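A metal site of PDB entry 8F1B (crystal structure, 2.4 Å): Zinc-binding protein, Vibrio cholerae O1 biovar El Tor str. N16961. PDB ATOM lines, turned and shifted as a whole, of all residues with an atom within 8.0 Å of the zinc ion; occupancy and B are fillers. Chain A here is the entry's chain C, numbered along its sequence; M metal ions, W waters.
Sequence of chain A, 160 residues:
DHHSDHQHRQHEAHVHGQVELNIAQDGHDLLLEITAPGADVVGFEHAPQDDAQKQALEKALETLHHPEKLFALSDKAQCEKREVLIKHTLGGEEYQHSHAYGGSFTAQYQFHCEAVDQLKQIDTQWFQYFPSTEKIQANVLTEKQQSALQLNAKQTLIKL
Of the 15 residues printed, 3 come within 4 Å of the zinc ion. The nearest printed residue that does not touch the zinc ion is Gly 103 (4.3 Å).
OE2 of Glu 45 sits close to N of Gly 103 (3.5 Å). The side-chain carboxylate (OE1) of Glu 45 sits at hydrogen-bond distance from the backbone NH (N) of Ala 39 (2.7 Å). The side-chain carboxylate (OE1) of Glu 45 is in hydrogen-bond range of the backbone NH (N) of Gly 38 (3.2 Å).
NE2 of His 14 binds the zinc ion, 1.9 Å away. The zinc ion is bound by OE2 of Glu 45 (2.0 Å). The zinc ion is bound by NE2 of His 16, at 2.0 Å. The zinc ion is bound by water W1, 2.1 Å away.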
ATOM      1  N   HIS A  14      28.861 -15.551   7.671  1.00  0.00           N
ATOM      2  CA  HIS A  14      27.600 -14.752   7.623  1.00  0.00           C
ATOM      3  C   HIS A  14      27.904 -13.314   8.007  1.00  0.00           C
ATOM      4  O   HIS A  14      28.033 -13.023   9.197  1.00  0.00           O
ATOM      5  CB  HIS A  14      26.551 -15.367   8.527  1.00  0.00           C
ATOM      6  CG  HIS A  14      25.243 -14.648   8.494  1.00  0.00           C
ATOM      7  ND1 HIS A  14      24.298 -14.862   7.523  1.00  0.00           N
ATOM      8  CD2 HIS A  14      24.723 -13.730   9.334  1.00  0.00           C
ATOM      9  CE1 HIS A  14      23.250 -14.109   7.754  1.00  0.00           C
ATOM     10  NE2 HIS A  14      23.488 -13.400   8.865  1.00  0.00           N
ATOM     11  N   VAL A  15      27.991 -12.457   6.999  1.00  0.00           N
ATOM     12  CA  VAL A  15      28.214 -10.999   7.134  1.00  0.00           C
ATOM     13  C   VAL A  15      27.213 -10.284   6.231  1.00  0.00           C
ATOM     14  O   VAL A  15      27.238 -10.533   5.010  1.00  0.00           O
ATOM     15  CB  VAL A  15      29.668 -10.665   6.735  1.00  0.00           C
ATOM     16  CG1 VAL A  15      29.977  -9.179   6.926  1.00  0.00           C
ATOM     17  CG2 VAL A  15      30.660 -11.550   7.480  1.00  0.00           C
ATOM     18  N   HIS A  16      26.401  -9.399   6.798  1.00  0.00           N
ATOM     19  CA  HIS A  16      25.399  -8.616   6.019  1.00  0.00           C
ATOM     20  C   HIS A  16      26.136  -7.769   4.976  1.00  0.00           C
ATOM     21  O   HIS A  16      27.150  -7.145   5.325  1.00  0.00           O
ATOM     22  CB  HIS A  16      24.486  -7.794   6.934  1.00  0.00           C
ATOM     23  CG  HIS A  16      23.702  -8.633   7.881  1.00  0.00           C
ATOM     24  ND1 HIS A  16      22.717  -8.115   8.696  1.00  0.00           N
ATOM     25  CD2 HIS A  16      23.746  -9.961   8.145  1.00  0.00           C
ATOM     26  CE1 HIS A  16      22.199  -9.096   9.436  1.00  0.00           C
ATOM     27  NE2 HIS A  16      22.832 -10.239   9.118  1.00  0.00           N
ATOM     28  N   ALA A  36      23.650 -16.396   0.848  1.00  0.00           N
ATOM     29  CA  ALA A  36      23.385 -14.960   1.048  1.00  0.00           C
ATOM     30  C   ALA A  36      22.669 -14.772   2.369  1.00  0.00           C
ATOM     31  O   ALA A  36      21.776 -15.533   2.744  1.00  0.00           O
ATOM     32  CB  ALA A  36      22.566 -14.421  -0.105  1.00  0.00           C
ATOM     33  N   PRO A  37      23.086 -13.750   3.145  1.00  0.00           N
ATOM     34  CA  PRO A  37      22.308 -13.369   4.319  1.00  0.00           C
ATOM     35  C   PRO A  37      20.908 -12.862   3.946  1.00  0.00           C
ATOM     36  O   PRO A  37      20.764 -12.139   2.971  1.00  0.00           O
ATOM     37  CB  PRO A  37      23.175 -12.256   4.919  1.00  0.00           C
ATOM     38  CG  PRO A  37      24.582 -12.538   4.413  1.00  0.00           C
ATOM     39  CD  PRO A  37      24.341 -12.992   2.996  1.00  0.00           C
ATOM     40  N   GLY A  38      19.900 -13.235   4.750  1.00  0.00           N
ATOM     41  CA  GLY A  38      18.511 -12.736   4.639  1.00  0.00           C
ATOM     42  C   GLY A  38      18.461 -11.228   4.509  1.00  0.00           C
ATOM     43  O   GLY A  38      17.642 -10.727   3.718  1.00  0.00           O
ATOM     44  N   ALA A  39      19.333 -10.516   5.225  1.00  0.00           N
ATOM     45  CA  ALA A  39      19.427  -9.038   5.137  1.00  0.00           C
ATOM     46  C   ALA A  39      19.666  -8.636   3.680  1.00  0.00           C
ATOM     47  O   ALA A  39      19.106  -7.605   3.226  1.00  0.00           O
ATOM     48  CB  ALA A  39      20.510  -8.518   6.039  1.00  0.00           C
ATOM     49  N   ASP A  40      20.490  -9.412   2.961  1.00  0.00           N
ATOM     50  CA  ASP A  40      20.829  -9.079   1.555  1.00  0.00           C
ATOM     51  C   ASP A  40      19.628  -9.352   0.653  1.00  0.00           C
ATOM     52  O   ASP A  40      19.309  -8.498  -0.197  1.00  0.00           O
ATOM     53  CB  ASP A  40      22.082  -9.802   1.088  1.00  0.00           C
ATOM     54  CG  ASP A  40      23.335  -9.157   1.621  1.00  0.00           C
ATOM     55  OD1 ASP A  40      23.367  -8.813   2.832  1.00  0.00           O
ATOM     56  OD2 ASP A  40      24.279  -9.018   0.840  1.00  0.00           O
ATOM     57  N   PHE A  44      15.742  -8.257   5.734  1.00  0.00           N
ATOM     58  CA  PHE A  44      15.524  -8.541   7.174  1.00  0.00           C
ATOM     59  C   PHE A  44      15.772 -10.031   7.418  1.00  0.00           C
ATOM     60  O   PHE A  44      15.809 -10.811   6.428  1.00  0.00           O
ATOM     61  CB  PHE A  44      14.120  -8.127   7.627  1.00  0.00           C
ATOM     62  CG  PHE A  44      13.017  -8.756   6.824  1.00  0.00           C
ATOM     63  CD1 PHE A  44      12.281  -9.818   7.326  1.00  0.00           C
ATOM     64  CD2 PHE A  44      12.756  -8.331   5.525  1.00  0.00           C
ATOM     65  CE1 PHE A  44      11.282 -10.406   6.573  1.00  0.00           C
ATOM     66  CE2 PHE A  44      11.769  -8.928   4.774  1.00  0.00           C
ATOM     67  CZ  PHE A  44      11.021  -9.962   5.298  1.00  0.00           C
ATOM     68  N   GLU A  45      15.958 -10.398   8.680  1.00  0.00           N
ATOM     69  CA  GLU A  45      16.278 -11.790   9.085  1.00  0.00           C
ATOM     70  C   GLU A  45      15.411 -12.162  10.275  1.00  0.00           C
ATOM     71  O   GLU A  45      15.938 -12.347  11.400  1.00  0.00           O
ATOM     72  CB  GLU A  45      17.776 -11.892   9.352  1.00  0.00           C
ATOM     73  CG  GLU A  45      18.584 -12.032   8.079  1.00  0.00           C
ATOM     74  CD  GLU A  45      20.058 -11.818   8.299  1.00  0.00           C
ATOM     75  OE1 GLU A  45      20.761 -11.479   7.342  1.00  0.00           O
ATOM     76  OE2 GLU A  45      20.440 -11.970   9.447  1.00  0.00           O
ATOM     77  N   LEU A  90      16.067 -19.663   8.937  1.00  0.00           N
ATOM     78  CA  LEU A  90      15.903 -18.512   9.856  1.00  0.00           C
ATOM     79  C   LEU A  90      16.385 -18.859  11.266  1.00  0.00           C
ATOM     80  O   LEU A  90      16.733 -17.914  11.992  1.00  0.00           O
ATOM     81  CB  LEU A  90      14.446 -18.047   9.807  1.00  0.00           C
ATOM     82  CG  LEU A  90      14.283 -16.536   9.946  1.00  0.00           C
ATOM     83  CD1 LEU A  90      15.454 -15.770   9.317  1.00  0.00           C
ATOM     84  CD2 LEU A  90      12.974 -16.073   9.323  1.00  0.00           C
ATOM     85  N   TYR A 101      16.362 -14.904  15.033  1.00  0.00           N
ATOM     86  CA  TYR A 101      17.069 -13.833  14.282  1.00  0.00           C
ATOM     87  C   TYR A 101      18.422 -14.390  13.826  1.00  0.00           C
ATOM     88  O   TYR A 101      19.238 -14.702  14.716  1.00  0.00           O
ATOM     89  CB  TYR A 101      17.210 -12.585  15.145  1.00  0.00           C
ATOM     90  CG  TYR A 101      17.858 -11.446  14.405  1.00  0.00           C
ATOM     91  CD1 TYR A 101      17.085 -10.525  13.723  1.00  0.00           C
ATOM     92  CD2 TYR A 101      19.240 -11.332  14.328  1.00  0.00           C
ATOM     93  CE1 TYR A 101      17.670  -9.487  13.008  1.00  0.00           C
ATOM     94  CE2 TYR A 101      19.838 -10.315  13.609  1.00  0.00           C
ATOM     95  CZ  TYR A 101      19.047  -9.389  12.948  1.00  0.00           C
ATOM     96  OH  TYR A 101      19.637  -8.366  12.249  1.00  0.00           O
ATOM     97  N   GLY A 102      18.618 -14.521  12.509  1.00  0.00           N
ATOM     98  CA  GLY A 102      19.856 -15.069  11.909  1.00  0.00           C
ATOM     99  C   GLY A 102      19.597 -15.829  10.615  1.00  0.00           C
ATOM    100  O   GLY A 102      19.983 -16.991  10.468  1.00  0.00           O
ATOM    101  N   GLY A 103      18.981 -15.143   9.655  1.00  0.00           N
ATOM    102  CA  GLY A 103      18.505 -15.748   8.428  1.00  0.00           C
ATOM    103  C   GLY A 103      19.582 -15.890   7.379  1.00  0.00           C
ATOM    104  O   GLY A 103      20.382 -14.985   7.204  1.00  0.00           O
ATOM    105  N   SER A 104      19.566 -17.004   6.657  1.00  0.00           N
ATOM    106  CA  SER A 104      20.439 -17.201   5.486  1.00  0.00           C
ATOM    107  C   SER A 104      19.635 -17.837   4.356  1.00  0.00           C
ATOM    108  O   SER A 104      18.687 -18.588   4.646  1.00  0.00           O
ATOM    109  CB  SER A 104      21.642 -18.002   5.821  1.00  0.00           C
ATOM    110  OG  SER A 104      22.725 -17.595   5.008  1.00  0.00           O
HETATM  111 ZN    ZN M   1      22.394 -12.103   9.727  1.00  0.00          ZN
HETATM  112  O   HOH W   1      22.575 -12.216  11.807  1.00  0.00           O
